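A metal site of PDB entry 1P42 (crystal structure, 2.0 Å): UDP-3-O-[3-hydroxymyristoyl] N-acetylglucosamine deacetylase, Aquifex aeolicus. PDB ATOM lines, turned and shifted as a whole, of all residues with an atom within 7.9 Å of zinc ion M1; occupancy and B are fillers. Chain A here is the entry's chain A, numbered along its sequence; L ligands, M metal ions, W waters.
Glu 72 touches zinc ion M1. Within 4 Å of zinc ion M1: Glu 72, His 73, His 225 and Asp 229.
Zinc ion M1 is bound by water W1 (1.8 Å), OD1 of Asp 229 (2.0 Å), NE2 of His 73 (2.1 Å) and NE2 of His 225 (2.2 Å). Zinc ion M1 has four donor atoms within binding distance. Slightly farther from zinc ion M1 lies the side-chain carboxylate (OD2) of Asp 229 (2.8 Å).
The side-chain carboxylate of Glu 72 is in hydrogen-bond range of the backbone NH of Thr 59 (2.9 Å). ND1 of His 225 sits close to N of Thr 178 (3.4 Å). A ring nitrogen (ND1) of His 225 sits close to the backbone carbonyl oxygen of Arg 177, at 3.4 Å. A ring nitrogen (ND1) of His 225 sits at hydrogen-bond distance from the backbone carbonyl oxygen (O) of Ala 176.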
ATOM      1  N   HIS A  57      16.395 -12.168  -0.583  1.00  0.00           N
ATOM      2  CA  HIS A  57      16.629 -10.759  -0.292  1.00  0.00           C
ATOM      3  C   HIS A  57      15.413  -9.894  -0.534  1.00  0.00           C
ATOM      4  O   HIS A  57      15.501  -8.667  -0.628  1.00  0.00           O
ATOM      5  CB  HIS A  57      17.830 -10.285  -1.115  1.00  0.00           C
ATOM      6  CG  HIS A  57      19.094 -11.016  -0.776  1.00  0.00           C
ATOM      7  ND1 HIS A  57      19.749 -10.850   0.422  1.00  0.00           N
ATOM      8  CD2 HIS A  57      19.767 -11.979  -1.448  1.00  0.00           C
ATOM      9  CE1 HIS A  57      20.773 -11.684   0.493  1.00  0.00           C
ATOM     10  NE2 HIS A  57      20.803 -12.382  -0.633  1.00  0.00           N
ATOM     11  N   SER A  58      14.264 -10.547  -0.621  1.00  0.00           N
ATOM     12  CA  SER A  58      12.976  -9.895  -0.833  1.00  0.00           C
ATOM     13  C   SER A  58      11.953 -11.009  -1.018  1.00  0.00           C
ATOM     14  O   SER A  58      12.326 -12.170  -1.153  1.00  0.00           O
ATOM     15  CB  SER A  58      13.020  -8.989  -2.074  1.00  0.00           C
ATOM     16  OG  SER A  58      13.307  -9.709  -3.261  1.00  0.00           O
ATOM     17  N   THR A  59      10.676 -10.660  -1.001  1.00  0.00           N
ATOM     18  CA  THR A  59       9.628 -11.652  -1.217  1.00  0.00           C
ATOM     19  C   THR A  59       9.141 -11.417  -2.638  1.00  0.00           C
ATOM     20  O   THR A  59       8.604 -10.348  -2.938  1.00  0.00           O
ATOM     21  CB  THR A  59       8.470 -11.472  -0.205  1.00  0.00           C
ATOM     22  OG1 THR A  59       8.986 -11.628   1.126  1.00  0.00           O
ATOM     23  CG2 THR A  59       7.391 -12.536  -0.440  1.00  0.00           C
ATOM     24  N   THR A  70       9.939  -7.988  -4.675  1.00  0.00           N
ATOM     25  CA  THR A  70       9.773  -7.111  -3.521  1.00  0.00           C
ATOM     26  C   THR A  70       8.361  -6.630  -3.214  1.00  0.00           C
ATOM     27  O   THR A  70       8.099  -5.419  -3.199  1.00  0.00           O
ATOM     28  CB  THR A  70      10.700  -5.881  -3.697  1.00  0.00           C
ATOM     29  OG1 THR A  70      11.937  -6.328  -4.260  1.00  0.00           O
ATOM     30  CG2 THR A  70      10.980  -5.189  -2.349  1.00  0.00           C
ATOM     31  N   GLU A  72       6.813  -7.306  -0.303  1.00  0.00           N
ATOM     32  CA  GLU A  72       6.608  -7.222   1.142  1.00  0.00           C
ATOM     33  C   GLU A  72       6.086  -5.914   1.747  1.00  0.00           C
ATOM     34  O   GLU A  72       5.284  -5.955   2.684  1.00  0.00           O
ATOM     35  CB  GLU A  72       7.874  -7.658   1.903  1.00  0.00           C
ATOM     36  CG  GLU A  72       9.115  -6.819   1.594  1.00  0.00           C
ATOM     37  CD  GLU A  72      10.032  -7.461   0.570  1.00  0.00           C
ATOM     38  OE1 GLU A  72       9.520  -8.018  -0.419  1.00  0.00           O
ATOM     39  OE2 GLU A  72      11.273  -7.379   0.732  1.00  0.00           O
ATOM     40  N   HIS A  73       6.532  -4.771   1.232  1.00  0.00           N
ATOM     41  CA  HIS A  73       6.109  -3.489   1.806  1.00  0.00           C
ATOM     42  C   HIS A  73       4.712  -3.041   1.400  1.00  0.00           C
ATOM     43  O   HIS A  73       3.942  -2.597   2.238  1.00  0.00           O
ATOM     44  CB  HIS A  73       7.149  -2.407   1.481  1.00  0.00           C
ATOM     45  CG  HIS A  73       8.519  -2.732   1.985  1.00  0.00           C
ATOM     46  ND1 HIS A  73       9.638  -2.024   1.614  1.00  0.00           N
ATOM     47  CD2 HIS A  73       8.954  -3.704   2.822  1.00  0.00           C
ATOM     48  CE1 HIS A  73      10.707  -2.537   2.191  1.00  0.00           C
ATOM     49  NE2 HIS A  73      10.320  -3.563   2.932  1.00  0.00           N
ATOM     50  N   SER A  76       2.348  -5.251   3.223  1.00  0.00           N
ATOM     51  CA  SER A  76       2.236  -4.990   4.653  1.00  0.00           C
ATOM     52  C   SER A  76       1.296  -3.807   4.911  1.00  0.00           C
ATOM     53  O   SER A  76       0.485  -3.840   5.830  1.00  0.00           O
ATOM     54  CB  SER A  76       3.607  -4.688   5.260  1.00  0.00           C
ATOM     55  OG  SER A  76       3.496  -4.513   6.668  1.00  0.00           O
ATOM     56  N   ILE A  97      10.769   0.880  -4.482  1.00  0.00           N
ATOM     57  CA  ILE A  97      11.179   0.857  -3.091  1.00  0.00           C
ATOM     58  C   ILE A  97      10.905   2.181  -2.375  1.00  0.00           C
ATOM     59  O   ILE A  97      10.744   2.214  -1.149  1.00  0.00           O
ATOM     60  CB  ILE A  97      12.706   0.529  -2.974  1.00  0.00           C
ATOM     61  CG1 ILE A  97      13.096   0.337  -1.508  1.00  0.00           C
ATOM     62  CG2 ILE A  97      13.539   1.637  -3.598  1.00  0.00           C
ATOM     63  CD1 ILE A  97      12.462  -0.870  -0.850  1.00  0.00           C
ATOM     64  N   GLY A 100      12.211   3.175   1.199  1.00  0.00           N
ATOM     65  CA  GLY A 100      12.567   1.981   1.944  1.00  0.00           C
ATOM     66  C   GLY A 100      11.565   1.566   3.013  1.00  0.00           C
ATOM     67  O   GLY A 100      11.717   0.520   3.635  1.00  0.00           O
ATOM     68  N   SER A 101      10.542   2.389   3.240  1.00  0.00           N
ATOM     69  CA  SER A 101       9.509   2.086   4.238  1.00  0.00           C
ATOM     70  C   SER A 101       8.139   2.007   3.554  1.00  0.00           C
ATOM     71  O   SER A 101       8.051   2.000   2.323  1.00  0.00           O
ATOM     72  CB  SER A 101       9.473   3.156   5.338  1.00  0.00           C
ATOM     73  OG  SER A 101       8.889   4.368   4.874  1.00  0.00           O
ATOM     74  N   ALA A 176       9.540   2.793   9.379  1.00  0.00           N
ATOM     75  CA  ALA A 176      10.803   2.078   9.528  1.00  0.00           C
ATOM     76  C   ALA A 176      11.308   1.610   8.165  1.00  0.00           C
ATOM     77  O   ALA A 176      10.619   0.881   7.447  1.00  0.00           O
ATOM     78  CB  ALA A 176      10.638   0.887  10.474  1.00  0.00           C
ATOM     79  N   ARG A 177      12.531   2.016   7.820  1.00  0.00           N
ATOM     80  CA  ARG A 177      13.135   1.684   6.541  1.00  0.00           C
ATOM     81  C   ARG A 177      13.890   0.370   6.500  1.00  0.00           C
ATOM     82  O   ARG A 177      14.385  -0.124   7.518  1.00  0.00           O
ATOM     83  CB  ARG A 177      14.102   2.790   6.122  1.00  0.00           C
ATOM     84  CG  ARG A 177      13.471   4.154   5.980  1.00  0.00           C
ATOM     85  CD  ARG A 177      14.562   5.201   5.997  1.00  0.00           C
ATOM     86  NE  ARG A 177      15.246   5.219   7.276  1.00  0.00           N
ATOM     87  CZ  ARG A 177      16.367   5.887   7.524  1.00  0.00           C
ATOM     88  NH1 ARG A 177      16.935   6.606   6.563  1.00  0.00           N
ATOM     89  NH2 ARG A 177      16.904   5.855   8.734  1.00  0.00           N
ATOM     90  N   THR A 178      13.989  -0.193   5.296  1.00  0.00           N
ATOM     91  CA  THR A 178      14.707  -1.432   5.075  1.00  0.00           C
ATOM     92  C   THR A 178      16.169  -1.104   5.383  1.00  0.00           C
ATOM     93  O   THR A 178      16.605   0.046   5.240  1.00  0.00           O
ATOM     94  CB  THR A 178      14.550  -1.900   3.610  1.00  0.00           C
ATOM     95  OG1 THR A 178      15.296  -3.099   3.405  1.00  0.00           O
ATOM     96  CG2 THR A 178      15.061  -0.839   2.650  1.00  0.00           C
ATOM     97  N   PHE A 179      16.936  -2.097   5.816  1.00  0.00           N
ATOM     98  CA  PHE A 179      18.331  -1.874   6.167  1.00  0.00           C
ATOM     99  C   PHE A 179      19.208  -3.025   5.725  1.00  0.00           C
ATOM    100  O   PHE A 179      18.719  -4.132   5.454  1.00  0.00           O
ATOM    101  CB  PHE A 179      18.451  -1.686   7.688  1.00  0.00           C
ATOM    102  CG  PHE A 179      18.101  -2.923   8.481  1.00  0.00           C
ATOM    103  CD1 PHE A 179      19.087  -3.824   8.874  1.00  0.00           C
ATOM    104  CD2 PHE A 179      16.773  -3.196   8.803  1.00  0.00           C
ATOM    105  CE1 PHE A 179      18.770  -4.982   9.568  1.00  0.00           C
ATOM    106  CE2 PHE A 179      16.436  -4.367   9.496  1.00  0.00           C
ATOM    107  CZ  PHE A 179      17.432  -5.260   9.883  1.00  0.00           C
ATOM    108  N   HIS A 225      11.292  -2.440  11.382  1.00  0.00           N
ATOM    109  CA  HIS A 225      11.147  -2.769   9.969  1.00  0.00           C
ATOM    110  C   HIS A 225      10.912  -4.263   9.786  1.00  0.00           C
ATOM    111  O   HIS A 225      10.147  -4.669   8.916  1.00  0.00           O
ATOM    112  CB  HIS A 225      12.378  -2.367   9.154  1.00  0.00           C
ATOM    113  CG  HIS A 225      12.172  -2.552   7.686  1.00  0.00           C
ATOM    114  ND1 HIS A 225      11.435  -1.665   6.919  1.00  0.00           N
ATOM    115  CD2 HIS A 225      12.508  -3.570   6.859  1.00  0.00           C
ATOM    116  CE1 HIS A 225      11.321  -2.137   5.695  1.00  0.00           C
ATOM    117  NE2 HIS A 225      11.965  -3.292   5.626  1.00  0.00           N
ATOM    118  N   LYS A 226      11.571  -5.084  10.609  1.00  0.00           N
ATOM    119  CA  LYS A 226      11.395  -6.525  10.509  1.00  0.00           C
ATOM    120  C   LYS A 226       9.954  -6.907  10.881  1.00  0.00           C
ATOM    121  O   LYS A 226       9.398  -7.849  10.313  1.00  0.00           O
ATOM    122  CB  LYS A 226      12.383  -7.248  11.421  1.00  0.00           C
ATOM    123  CG  LYS A 226      13.815  -7.252  10.900  1.00  0.00           C
ATOM    124  CD  LYS A 226      13.949  -8.018   9.593  1.00  0.00           C
ATOM    125  CE  LYS A 226      15.392  -8.036   9.103  1.00  0.00           C
ATOM    126  NZ  LYS A 226      15.570  -8.798   7.835  1.00  0.00           N
ATOM    127  N   PHE A 228       7.431  -4.965  10.346  1.00  0.00           N
ATOM    128  CA  PHE A 228       6.720  -4.489   9.167  1.00  0.00           C
ATOM    129  C   PHE A 228       6.800  -5.543   8.058  1.00  0.00           C
ATOM    130  O   PHE A 228       5.789  -5.824   7.395  1.00  0.00           O
ATOM    131  CB  PHE A 228       7.348  -3.164   8.714  1.00  0.00           C
ATOM    132  CG  PHE A 228       6.717  -2.566   7.489  1.00  0.00           C
ATOM    133  CD1 PHE A 228       5.403  -2.081   7.527  1.00  0.00           C
ATOM    134  CD2 PHE A 228       7.443  -2.457   6.300  1.00  0.00           C
ATOM    135  CE1 PHE A 228       4.832  -1.501   6.399  1.00  0.00           C
ATOM    136  CE2 PHE A 228       6.870  -1.873   5.158  1.00  0.00           C
ATOM    137  CZ  PHE A 228       5.558  -1.392   5.210  1.00  0.00           C
ATOM    138  N   ASP A 229       7.973  -6.137   7.862  1.00  0.00           N
ATOM    139  CA  ASP A 229       8.152  -7.179   6.840  1.00  0.00           C
ATOM    140  C   ASP A 229       7.292  -8.410   7.118  1.00  0.00           C
ATOM    141  O   ASP A 229       6.650  -8.940   6.211  1.00  0.00           O
ATOM    142  CB  ASP A 229       9.605  -7.655   6.784  1.00  0.00           C
ATOM    143  CG  ASP A 229      10.509  -6.706   6.043  1.00  0.00           C
ATOM    144  OD1 ASP A 229      10.001  -5.884   5.257  1.00  0.00           O
ATOM    145  OD2 ASP A 229      11.737  -6.806   6.237  1.00  0.00           O
ATOM    146  N   LEU A 230       7.313  -8.893   8.355  1.00  0.00           N
ATOM    147  CA  LEU A 230       6.550 -10.076   8.717  1.00  0.00           C
ATOM    148  C   LEU A 230       5.056  -9.875   8.469  1.00  0.00           C
ATOM    149  O   LEU A 230       4.371 -10.777   7.972  1.00  0.00           O
ATOM    150  CB  LEU A 230       6.807 -10.425  10.195  1.00  0.00           C
ATOM    151  CG  LEU A 230       6.031 -11.602  10.810  1.00  0.00           C
ATOM    152  CD1 LEU A 230       6.110 -12.837   9.920  1.00  0.00           C
ATOM    153  CD2 LEU A 230       6.603 -11.885  12.180  1.00  0.00           C
ATOM    154  N   ASP A 233       4.505 -10.327   4.840  1.00  0.00           N
ATOM    155  CA  ASP A 233       4.564 -11.728   4.440  1.00  0.00           C
ATOM    156  C   ASP A 233       3.362 -12.522   4.938  1.00  0.00           C
ATOM    157  O   ASP A 233       2.890 -13.445   4.281  1.00  0.00           O
ATOM    158  CB  ASP A 233       5.866 -12.378   4.921  1.00  0.00           C
ATOM    159  CG  ASP A 233       7.094 -11.873   4.149  1.00  0.00           C
ATOM    160  OD1 ASP A 233       6.950 -11.507   2.967  1.00  0.00           O
ATOM    161  OD2 ASP A 233       8.209 -11.855   4.731  1.00  0.00           O
ATOM    162  N   HIS A 252      12.356 -13.138   5.539  1.00  0.00           N
ATOM    163  CA  HIS A 252      11.341 -13.524   4.556  1.00  0.00           C
ATOM    164  C   HIS A 252      11.251 -15.035   4.359  1.00  0.00           C
ATOM    165  O   HIS A 252      10.163 -15.574   4.248  1.00  0.00           O
ATOM    166  CB  HIS A 252      11.615 -12.840   3.205  1.00  0.00           C
ATOM    167  CG  HIS A 252      11.510 -11.351   3.266  1.00  0.00           C
ATOM    168  ND1 HIS A 252      10.376 -10.703   3.700  1.00  0.00           N
ATOM    169  CD2 HIS A 252      12.405 -10.386   2.946  1.00  0.00           C
ATOM    170  CE1 HIS A 252      10.574  -9.394   3.662  1.00  0.00           C
ATOM    171  NE2 HIS A 252      11.804  -9.177   3.207  1.00  0.00           N
HETATM  172  C1  LIG L   1      15.410  -8.035   2.609  1.00  0.00           C
HETATM  173  O1  LIG L   1      14.453  -7.755   1.824  1.00  0.00           O
HETATM  174  O2  LIG L   1      15.293  -8.752   3.645  1.00  0.00           O
HETATM  175  C2  LIG L   1      16.821  -7.491   2.274  1.00  0.00           C
HETATM  176  C3  LIG L   1      16.878  -5.984   2.331  1.00  0.00           C
HETATM  177  C4  LIG L   1      18.221  -5.476   1.859  1.00  0.00           C
HETATM  178  C5  LIG L   1      18.132  -4.907   0.457  1.00  0.00           C
HETATM  179  C6  LIG L   1      19.507  -4.777  -0.175  1.00  0.00           C
HETATM  180  C7  LIG L   1      19.866  -3.325  -0.387  1.00  0.00           C
HETATM  181  C8  LIG L   1      20.778  -3.150  -1.589  1.00  0.00           C
HETATM  182  C9  LIG L   1      22.172  -2.712  -1.197  1.00  0.00           C
HETATM  183  C10 LIG L   1      22.207  -1.243  -0.833  1.00  0.00           C
HETATM  184  C11 LIG L   1      23.459  -0.553  -1.321  1.00  0.00           C
HETATM  185  C12 LIG L   1      23.725   0.699  -0.530  1.00  0.00           C
HETATM  186  C13 LIG L   1      24.591   1.680  -1.284  1.00  0.00           C
HETATM  187  C14 LIG L   1      26.039   1.607  -0.844  1.00  0.00           C
HETATM  188 ZN    ZN M   1      11.348  -4.834   4.227  1.00  0.00          ZN
HETATM  189 ZN    ZN M   2      12.426  -7.479   2.338  1.00  0.00          ZN
HETATM  190  O   HOH W   1      12.703  -5.648   3.358  1.00  0.00           O
